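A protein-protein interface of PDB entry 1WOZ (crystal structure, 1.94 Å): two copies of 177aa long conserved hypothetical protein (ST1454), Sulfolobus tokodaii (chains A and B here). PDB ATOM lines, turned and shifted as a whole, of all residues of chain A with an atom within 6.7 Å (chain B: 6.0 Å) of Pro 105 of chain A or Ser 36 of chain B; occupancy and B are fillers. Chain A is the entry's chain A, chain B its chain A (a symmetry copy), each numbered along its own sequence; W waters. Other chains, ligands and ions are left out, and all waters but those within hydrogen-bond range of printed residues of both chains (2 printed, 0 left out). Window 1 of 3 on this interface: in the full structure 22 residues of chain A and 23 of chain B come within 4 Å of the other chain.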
ATOM      1  N   VAL A 103     -14.860  23.922  22.963  1.00  0.00           N
ATOM      2  CA  VAL A 103     -16.025  24.422  22.255  1.00  0.00           C
ATOM      3  C   VAL A 103     -17.094  24.702  23.329  1.00  0.00           C
ATOM      4  O   VAL A 103     -17.356  23.857  24.189  1.00  0.00           O
ATOM      5  CB  VAL A 103     -16.561  23.368  21.243  1.00  0.00           C
ATOM      6  CG1 VAL A 103     -17.996  23.724  20.808  1.00  0.00           C
ATOM      7  CG2 VAL A 103     -15.632  23.320  20.033  1.00  0.00           C
ATOM      8  N   ILE A 104     -17.675  25.900  23.295  1.00  0.00           N
ATOM      9  CA  ILE A 104     -18.739  26.266  24.237  1.00  0.00           C
ATOM     10  C   ILE A 104     -19.990  25.667  23.607  1.00  0.00           C
ATOM     11  O   ILE A 104     -20.379  26.037  22.487  1.00  0.00           O
ATOM     12  CB  ILE A 104     -18.866  27.796  24.359  1.00  0.00           C
ATOM     13  CG1 ILE A 104     -17.576  28.358  24.993  1.00  0.00           C
ATOM     14  CG2 ILE A 104     -20.129  28.154  25.198  1.00  0.00           C
ATOM     15  CD1 ILE A 104     -17.528  29.907  25.107  1.00  0.00           C
ATOM     16  N   PRO A 105     -20.650  24.736  24.317  1.00  0.00           N
ATOM     17  CA  PRO A 105     -21.840  24.099  23.752  1.00  0.00           C
ATOM     18  C   PRO A 105     -22.991  25.018  23.346  1.00  0.00           C
ATOM     19  O   PRO A 105     -23.471  25.828  24.143  1.00  0.00           O
ATOM     20  CB  PRO A 105     -22.226  23.070  24.831  1.00  0.00           C
ATOM     21  CG  PRO A 105     -21.789  23.733  26.096  1.00  0.00           C
ATOM     22  CD  PRO A 105     -20.441  24.323  25.719  1.00  0.00           C
ATOM     23  N   GLY A 106     -23.426  24.871  22.094  1.00  0.00           N
ATOM     24  CA  GLY A 106     -24.512  25.704  21.598  1.00  0.00           C
ATOM     25  C   GLY A 106     -24.394  26.005  20.104  1.00  0.00           C
ATOM     26  O   GLY A 106     -23.730  25.270  19.355  1.00  0.00           O
ATOM     27  N   GLY A 107     -25.045  27.092  19.694  1.00  0.00           N
ATOM     28  CA  GLY A 107     -25.059  27.534  18.304  1.00  0.00           C
ATOM     29  C   GLY A 107     -26.435  27.304  17.689  1.00  0.00           C
ATOM     30  O   GLY A 107     -27.443  27.864  18.160  1.00  0.00           O
ATOM     31  N   ALA A 111     -27.158  21.736  16.738  1.00  0.00           N
ATOM     32  CA  ALA A 111     -25.929  21.503  17.488  1.00  0.00           C
ATOM     33  C   ALA A 111     -26.214  21.579  19.001  1.00  0.00           C
ATOM     34  O   ALA A 111     -25.627  20.833  19.788  1.00  0.00           O
ATOM     35  CB  ALA A 111     -24.867  22.545  17.114  1.00  0.00           C
ATOM     36  N   SER A 112     -27.112  22.473  19.405  1.00  0.00           N
ATOM     37  CA  SER A 112     -27.400  22.617  20.832  1.00  0.00           C
ATOM     38  C   SER A 112     -28.029  21.358  21.405  1.00  0.00           C
ATOM     39  O   SER A 112     -27.649  20.928  22.492  1.00  0.00           O
ATOM     40  CB  SER A 112     -28.327  23.818  21.095  1.00  0.00           C
ATOM     41  OG  SER A 112     -27.685  25.030  20.725  1.00  0.00           O
ATOM     42  N   VAL A 113     -28.982  20.760  20.689  1.00  0.00           N
ATOM     43  CA  VAL A 113     -29.602  19.550  21.211  1.00  0.00           C
ATOM     44  C   VAL A 113     -28.605  18.397  21.215  1.00  0.00           C
ATOM     45  O   VAL A 113     -28.656  17.521  22.098  1.00  0.00           O
ATOM     46  CB  VAL A 113     -30.879  19.176  20.436  1.00  0.00           C
ATOM     47  CG1 VAL A 113     -31.545  17.955  21.090  1.00  0.00           C
ATOM     48  CG2 VAL A 113     -31.861  20.336  20.489  1.00  0.00           C
ATOM     49  N   HIS A 115     -25.374  18.740  21.771  1.00  0.00           N
ATOM     50  CA  HIS A 115     -24.508  18.956  22.925  1.00  0.00           C
ATOM     51  C   HIS A 115     -25.208  18.543  24.220  1.00  0.00           C
ATOM     52  O   HIS A 115     -24.573  18.033  25.148  1.00  0.00           O
ATOM     53  CB  HIS A 115     -24.080  20.428  23.027  1.00  0.00           C
ATOM     54  CG  HIS A 115     -22.905  20.758  22.167  1.00  0.00           C
ATOM     55  ND1 HIS A 115     -21.680  20.149  22.332  1.00  0.00           N
ATOM     56  CD2 HIS A 115     -22.768  21.614  21.122  1.00  0.00           C
ATOM     57  CE1 HIS A 115     -20.837  20.610  21.423  1.00  0.00           C
ATOM     58  NE2 HIS A 115     -21.472  21.500  20.677  1.00  0.00           N
ATOM     59  N   VAL A 116     -26.512  18.801  24.310  1.00  0.00           N
ATOM     60  CA  VAL A 116     -27.229  18.381  25.509  1.00  0.00           C
ATOM     61  C   VAL A 116     -27.168  16.846  25.589  1.00  0.00           C
ATOM     62  O   VAL A 116     -26.901  16.264  26.649  1.00  0.00           O
ATOM     63  CB  VAL A 116     -28.718  18.813  25.464  1.00  0.00           C
ATOM     64  CG1 VAL A 116     -29.516  18.028  26.512  1.00  0.00           C
ATOM     65  CG2 VAL A 116     -28.839  20.332  25.705  1.00  0.00           C
ATOM     66  N   THR A 117     -27.417  16.203  24.456  1.00  0.00           N
ATOM     67  CA  THR A 117     -27.402  14.747  24.379  1.00  0.00           C
ATOM     68  C   THR A 117     -25.998  14.236  24.737  1.00  0.00           C
ATOM     69  O   THR A 117     -25.845  13.258  25.480  1.00  0.00           O
ATOM     70  CB  THR A 117     -27.836  14.314  22.960  1.00  0.00           C
ATOM     71  OG1 THR A 117     -29.133  14.871  22.704  1.00  0.00           O
ATOM     72  CG2 THR A 117     -27.932  12.791  22.842  1.00  0.00           C
ATOM     73  N   ARG A 118     -24.975  14.934  24.243  1.00  0.00           N
ATOM     74  CA  ARG A 118     -23.590  14.590  24.541  1.00  0.00           C
ATOM     75  C   ARG A 118     -23.309  14.658  26.068  1.00  0.00           C
ATOM     76  O   ARG A 118     -22.671  13.768  26.662  1.00  0.00           O
ATOM     77  CB  ARG A 118     -22.676  15.567  23.768  1.00  0.00           C
ATOM     78  CG  ARG A 118     -21.159  15.479  24.051  1.00  0.00           C
ATOM     79  CD  ARG A 118     -20.418  16.753  23.505  1.00  0.00           C
ATOM     80  NE  ARG A 118     -20.906  17.963  24.180  1.00  0.00           N
ATOM     81  CZ  ARG A 118     -20.673  18.263  25.452  1.00  0.00           C
ATOM     82  NH1 ARG A 118     -19.917  17.461  26.210  1.00  0.00           N
ATOM     83  NH2 ARG A 118     -21.281  19.314  26.002  1.00  0.00           N
ATOM     84  N   SER A 119     -23.783  15.708  26.715  1.00  0.00           N
ATOM     85  CA  SER A 119     -23.551  15.847  28.161  1.00  0.00           C
ATOM     86  C   SER A 119     -24.295  14.770  28.958  1.00  0.00           C
ATOM     87  O   SER A 119     -23.824  14.320  30.016  1.00  0.00           O
ATOM     88  CB  SER A 119     -23.932  17.258  28.635  1.00  0.00           C
ATOM     89  OG  SER A 119     -25.328  17.457  28.618  1.00  0.00           O
ATOM     90  N   GLU A 168     -18.508  28.414  15.759  1.00  0.00           N
ATOM     91  CA  GLU A 168     -18.341  27.830  17.077  1.00  0.00           C
ATOM     92  C   GLU A 168     -17.856  28.912  18.040  1.00  0.00           C
ATOM     93  O   GLU A 168     -17.052  29.775  17.664  1.00  0.00           O
ATOM     94  CB  GLU A 168     -17.282  26.729  17.045  1.00  0.00           C
ATOM     95  CG  GLU A 168     -17.612  25.555  16.138  1.00  0.00           C
ATOM     96  CD  GLU A 168     -18.862  24.827  16.577  1.00  0.00           C
ATOM     97  OE1 GLU A 168     -19.185  24.890  17.779  1.00  0.00           O
ATOM     98  OE2 GLU A 168     -19.505  24.184  15.724  1.00  0.00           O
ATOM     99  N   LYS A 169     -18.355  28.871  19.270  1.00  0.00           N
ATOM    100  CA  LYS A 169     -17.917  29.800  20.310  1.00  0.00           C
ATOM    101  C   LYS A 169     -16.831  28.998  21.035  1.00  0.00           C
ATOM    102  O   LYS A 169     -17.033  27.837  21.328  1.00  0.00           O
ATOM    103  CB  LYS A 169     -19.045  30.099  21.296  1.00  0.00           C
ATOM    104  CG  LYS A 169     -20.351  30.529  20.649  1.00  0.00           C
ATOM    105  CD  LYS A 169     -20.301  31.952  20.156  1.00  0.00           C
ATOM    106  CE  LYS A 169     -21.707  32.419  19.721  1.00  0.00           C
ATOM    107  NZ  LYS A 169     -21.735  33.873  19.474  1.00  0.00           N
ATOM    108  N   LEU B  31     -21.410  20.644  35.432  1.00  0.00           N
ATOM    109  CA  LEU B  31     -21.266  21.985  34.878  1.00  0.00           C
ATOM    110  C   LEU B  31     -21.469  21.947  33.371  1.00  0.00           C
ATOM    111  O   LEU B  31     -22.105  22.826  32.801  1.00  0.00           O
ATOM    112  CB  LEU B  31     -19.882  22.565  35.211  1.00  0.00           C
ATOM    113  CG  LEU B  31     -19.802  22.928  36.694  1.00  0.00           C
ATOM    114  CD1 LEU B  31     -18.357  23.206  37.067  1.00  0.00           C
ATOM    115  CD2 LEU B  31     -20.690  24.146  36.993  1.00  0.00           C
ATOM    116  N   ASP B  32     -20.914  20.925  32.724  1.00  0.00           N
ATOM    117  CA  ASP B  32     -21.066  20.780  31.271  1.00  0.00           C
ATOM    118  C   ASP B  32     -22.548  20.539  30.898  1.00  0.00           C
ATOM    119  O   ASP B  32     -23.062  21.113  29.929  1.00  0.00           O
ATOM    120  CB  ASP B  32     -20.177  19.624  30.774  1.00  0.00           C
ATOM    121  CG  ASP B  32     -20.343  19.344  29.280  1.00  0.00           C
ATOM    122  OD1 ASP B  32     -20.407  20.293  28.478  1.00  0.00           O
ATOM    123  OD2 ASP B  32     -20.394  18.159  28.904  1.00  0.00           O
ATOM    124  N   GLU B  33     -23.231  19.688  31.660  1.00  0.00           N
ATOM    125  CA  GLU B  33     -24.640  19.429  31.374  1.00  0.00           C
ATOM    126  C   GLU B  33     -25.418  20.745  31.496  1.00  0.00           C
ATOM    127  O   GLU B  33     -26.222  21.093  30.633  1.00  0.00           O
ATOM    128  CB  GLU B  33     -25.201  18.355  32.327  1.00  0.00           C
ATOM    129  CG  GLU B  33     -26.659  18.004  31.989  1.00  0.00           C
ATOM    130  CD  GLU B  33     -27.260  16.887  32.844  1.00  0.00           C
ATOM    131  OE1 GLU B  33     -26.538  16.267  33.644  1.00  0.00           O
ATOM    132  OE2 GLU B  33     -28.474  16.615  32.696  1.00  0.00           O
ATOM    133  N   LEU B  34     -25.182  21.493  32.567  1.00  0.00           N
ATOM    134  CA  LEU B  34     -25.857  22.785  32.718  1.00  0.00           C
ATOM    135  C   LEU B  34     -25.498  23.722  31.546  1.00  0.00           C
ATOM    136  O   LEU B  34     -26.369  24.357  30.942  1.00  0.00           O
ATOM    137  CB  LEU B  34     -25.457  23.440  34.051  1.00  0.00           C
ATOM    138  CG  LEU B  34     -25.879  24.915  34.241  1.00  0.00           C
ATOM    139  CD1 LEU B  34     -27.411  25.051  34.191  1.00  0.00           C
ATOM    140  CD2 LEU B  34     -25.371  25.421  35.609  1.00  0.00           C
ATOM    141  N   ASN B  35     -24.214  23.783  31.212  1.00  0.00           N
ATOM    142  CA  ASN B  35     -23.745  24.649  30.132  1.00  0.00           C
ATOM    143  C   ASN B  35     -24.429  24.291  28.801  1.00  0.00           C
ATOM    144  O   ASN B  35     -24.756  25.171  27.991  1.00  0.00           O
ATOM    145  CB  ASN B  35     -22.208  24.508  30.012  1.00  0.00           C
ATOM    146  CG  ASN B  35     -21.530  25.780  29.501  1.00  0.00           C
ATOM    147  OD1 ASN B  35     -22.149  26.836  29.394  1.00  0.00           O
ATOM    148  ND2 ASN B  35     -20.249  25.673  29.189  1.00  0.00           N
ATOM    149  N   SER B  36     -24.648  22.994  28.577  1.00  0.00           N
ATOM    150  CA  SER B  36     -25.280  22.541  27.342  1.00  0.00           C
ATOM    151  C   SER B  36     -26.755  22.937  27.324  1.00  0.00           C
ATOM    152  O   SER B  36     -27.261  23.385  26.286  1.00  0.00           O
ATOM    153  CB  SER B  36     -25.098  21.028  27.175  1.00  0.00           C
ATOM    154  OG  SER B  36     -23.697  20.718  27.092  1.00  0.00           O
ATOM    155  N   PHE B  37     -27.460  22.791  28.452  1.00  0.00           N
ATOM    156  CA  PHE B  37     -28.861  23.257  28.467  1.00  0.00           C
ATOM    157  C   PHE B  37     -28.911  24.781  28.233  1.00  0.00           C
ATOM    158  O   PHE B  37     -29.826  25.299  27.571  1.00  0.00           O
ATOM    159  CB  PHE B  37     -29.556  22.898  29.796  1.00  0.00           C
ATOM    160  CG  PHE B  37     -30.139  21.494  29.818  1.00  0.00           C
ATOM    161  CD1 PHE B  37     -31.341  21.213  29.173  1.00  0.00           C
ATOM    162  CD2 PHE B  37     -29.448  20.447  30.431  1.00  0.00           C
ATOM    163  CE1 PHE B  37     -31.852  19.899  29.131  1.00  0.00           C
ATOM    164  CE2 PHE B  37     -29.932  19.126  30.397  1.00  0.00           C
ATOM    165  CZ  PHE B  37     -31.142  18.844  29.742  1.00  0.00           C
ATOM    166  N   ILE B  38     -27.942  25.513  28.775  1.00  0.00           N
ATOM    167  CA  ILE B  38     -27.937  26.959  28.547  1.00  0.00           C
ATOM    168  C   ILE B  38     -27.752  27.238  27.047  1.00  0.00           C
ATOM    169  O   ILE B  38     -28.416  28.109  26.485  1.00  0.00           O
ATOM    170  CB  ILE B  38     -26.825  27.664  29.355  1.00  0.00           C
ATOM    171  CG1 ILE B  38     -27.249  27.746  30.826  1.00  0.00           C
ATOM    172  CG2 ILE B  38     -26.613  29.097  28.832  1.00  0.00           C
ATOM    173  CD1 ILE B  38     -26.124  28.131  31.804  1.00  0.00           C
ATOM    174  N   GLY B  39     -26.859  26.480  26.405  1.00  0.00           N
ATOM    175  CA  GLY B  39     -26.634  26.643  24.981  1.00  0.00           C
ATOM    176  C   GLY B  39     -27.941  26.382  24.245  1.00  0.00           C
ATOM    177  O   GLY B  39     -28.258  27.086  23.280  1.00  0.00           O
ATOM    178  N   PHE B  40     -28.705  25.380  24.697  1.00  0.00           N
ATOM    179  CA  PHE B  40     -29.998  25.054  24.063  1.00  0.00           C
ATOM    180  C   PHE B  40     -30.994  26.211  24.290  1.00  0.00           C
ATOM    181  O   PHE B  40     -31.674  26.655  23.362  1.00  0.00           O
ATOM    182  CB  PHE B  40     -30.535  23.711  24.624  1.00  0.00           C
ATOM    183  CG  PHE B  40     -31.876  23.282  24.050  1.00  0.00           C
ATOM    184  CD1 PHE B  40     -32.924  22.925  24.896  1.00  0.00           C
ATOM    185  CD2 PHE B  40     -32.080  23.212  22.672  1.00  0.00           C
ATOM    186  CE1 PHE B  40     -34.162  22.500  24.386  1.00  0.00           C
ATOM    187  CE2 PHE B  40     -33.318  22.789  22.148  1.00  0.00           C
ATOM    188  CZ  PHE B  40     -34.352  22.434  23.009  1.00  0.00           C
ATOM    189  N   ALA B  41     -31.057  26.741  25.507  1.00  0.00           N
ATOM    190  CA  ALA B  41     -31.968  27.873  25.781  1.00  0.00           C
ATOM    191  C   ALA B  41     -31.628  29.072  24.866  1.00  0.00           C
ATOM    192  O   ALA B  41     -32.526  29.731  24.301  1.00  0.00           O
ATOM    193  CB  ALA B  41     -31.844  28.297  27.202  1.00  0.00           C
ATOM    194  N   GLN B  58     -22.122  31.102  30.130  1.00  0.00           N
ATOM    195  CA  GLN B  58     -21.411  29.924  29.616  1.00  0.00           C
ATOM    196  C   GLN B  58     -19.885  30.074  29.761  1.00  0.00           C
ATOM    197  O   GLN B  58     -19.180  29.139  30.143  1.00  0.00           O
ATOM    198  CB  GLN B  58     -21.742  29.693  28.154  1.00  0.00           C
ATOM    199  CG  GLN B  58     -23.201  29.399  27.868  1.00  0.00           C
ATOM    200  CD  GLN B  58     -23.348  28.898  26.459  1.00  0.00           C
ATOM    201  OE1 GLN B  58     -23.236  29.660  25.512  1.00  0.00           O
ATOM    202  NE2 GLN B  58     -23.557  27.593  26.313  1.00  0.00           N
ATOM    203  N   PHE B  62     -17.139  27.947  32.348  1.00  0.00           N
ATOM    204  CA  PHE B  62     -15.814  27.384  32.036  1.00  0.00           C
ATOM    205  C   PHE B  62     -14.814  27.932  33.058  1.00  0.00           C
ATOM    206  O   PHE B  62     -13.910  27.227  33.493  1.00  0.00           O
ATOM    207  CB  PHE B  62     -15.358  27.746  30.616  1.00  0.00           C
ATOM    208  CG  PHE B  62     -15.826  26.773  29.570  1.00  0.00           C
ATOM    209  CD1 PHE B  62     -17.042  26.948  28.923  1.00  0.00           C
ATOM    210  CD2 PHE B  62     -15.061  25.643  29.264  1.00  0.00           C
ATOM    211  CE1 PHE B  62     -17.498  26.007  27.986  1.00  0.00           C
ATOM    212  CE2 PHE B  62     -15.517  24.706  28.327  1.00  0.00           C
ATOM    213  CZ  PHE B  62     -16.742  24.900  27.693  1.00  0.00           C
HETATM  214  O   HOH W   1     -26.449  28.518  21.698  1.00  0.00           O
HETATM  215  O   HOH W   2     -26.086  23.102  23.853  1.00  0.00           O
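NE2 of Gln 58 of chain B lies within hydrogen-bond range of O of Pro 105 of chain A, 2.8 Å away. The side-chain hydroxyl (OG) of Ser 112 of chain A sits at hydrogen-bond distance from the backbone carbonyl oxygen (O) of Gly 39 of chain B (3.3 Å). The backbone carbonyl oxygen (O) of His 115 of chain A sits at hydrogen-bond distance from the side-chain hydroxyl (OG) of Ser 36 of chain B (3.4 Å). The side-chain carboxylate of Asp 32 of chain B is in salt-bridge range of the guanidinium group of Arg 118 of chain A. NH2 of Arg 118 of chain A sits at hydrogen-bond distance from OG of Ser 36 of chain B, 3.0 Å away.
N of Ile 104 of chain A is in hydrogen-bond range of O of Lys 169 of chain A (2.8 Å). The backbone carbonyl oxygen of Val 113 of chain A lies within hydrogen-bond range of the side-chain hydroxyl of Thr 117 of chain A, at 2.8 Å. ND1 of His 115 of chain A sits at hydrogen-bond distance from NE of Arg 118 of chain A. The backbone carbonyl oxygen of Val 116 of chain A is in hydrogen-bond range of the side-chain hydroxyl of Ser 119 of chain A (2.8 Å). NE2 of Gln 58 of chain B is in hydrogen-bond range of O of Asn 35 of chain B, at 3.2 Å. The side-chain amide nitrogen (NE2) of Gln 58 of chain B sits close to the backbone NH (N) of Gly 39 of chain B.
Among the printed residues, pairs that only touch across the chains: Val 113 of chain A with Phe 40 of chain B, Pro 105 of chain A with Gly 39 of chain B, Ser 119 of chain A with Glu 33 of chain B, Ile 104 of chain A with Gln 58 of chain B, Val 116 of chain A with Ser 36 of chain B, Pro 105 of chain A with Ser 36 of chain B, Ser 112 of chain A with Phe 40 of chain B, Ser 119 of chain A with Asp 32 of chain B, Val 116 of chain A with Phe 37 of chain B, Val 103 of chain A with Phe 62 of chain B, Pro 105 of chain A with Asn 35 of chain B, Ser 119 of chain A with Ser 36 of chain B, Ile 104 of chain A with Phe 62 of chain B and Val 116 of chain A with Phe 40 of chain B.
Ser 36 of chain B touches five residues of chain A. Of the printed residues of chain B, Val 116 of chain A touches Ser 36, Phe 37 and Phe 40. Printed residues of chain A within 4 Å of Phe 62 of chain B: Val 103 (3.7 Å) and Ile 104 (3.8 Å). Printed residues of chain A within 4 Å of Phe 37 of chain B: Val 116 (3.7 Å). Printed residues of chain A within 4 Å of Gln 58 of chain B: Ile 104 (3.5 Å) and Pro 105 (2.8 Å). Of the printed residues of chain A, Phe 40 of chain B touches Ser 112 (3.6 Å), Val 113 (3.3 Å) and Val 116 (3.9 Å). Gly 106 of chain A touches none of the printed residues of chain B. The nearest residue of chain B that does not touch Pro 105 of chain A is Phe 62 of chain B (4.1 Å). The nearest residue of chain A that does not touch Ser 36 of chain B is Ser 112 of chain A (4.5 Å).
Along chain A the printed residues that touch a printed residue of chain B span positions 103 to 119. Among the printed residues, Asp or Glu carboxylates within 4 Å of a Lys or Arg side-chain nitrogen of the other chain: Arg 118 of chain A with Asp 32 of chain B (2.8 Å).
No position is printed for both chains.
Water W2 lies within hydrogen-bond range of O of Ser 36 of chain B (2.7 Å) and O of Ser 112 of chain A (3.0 Å). Water W1 lies within hydrogen-bond range of O of Gly 39 of chain B (2.8 Å) and N of Gly 107 of chain A (2.8 Å).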
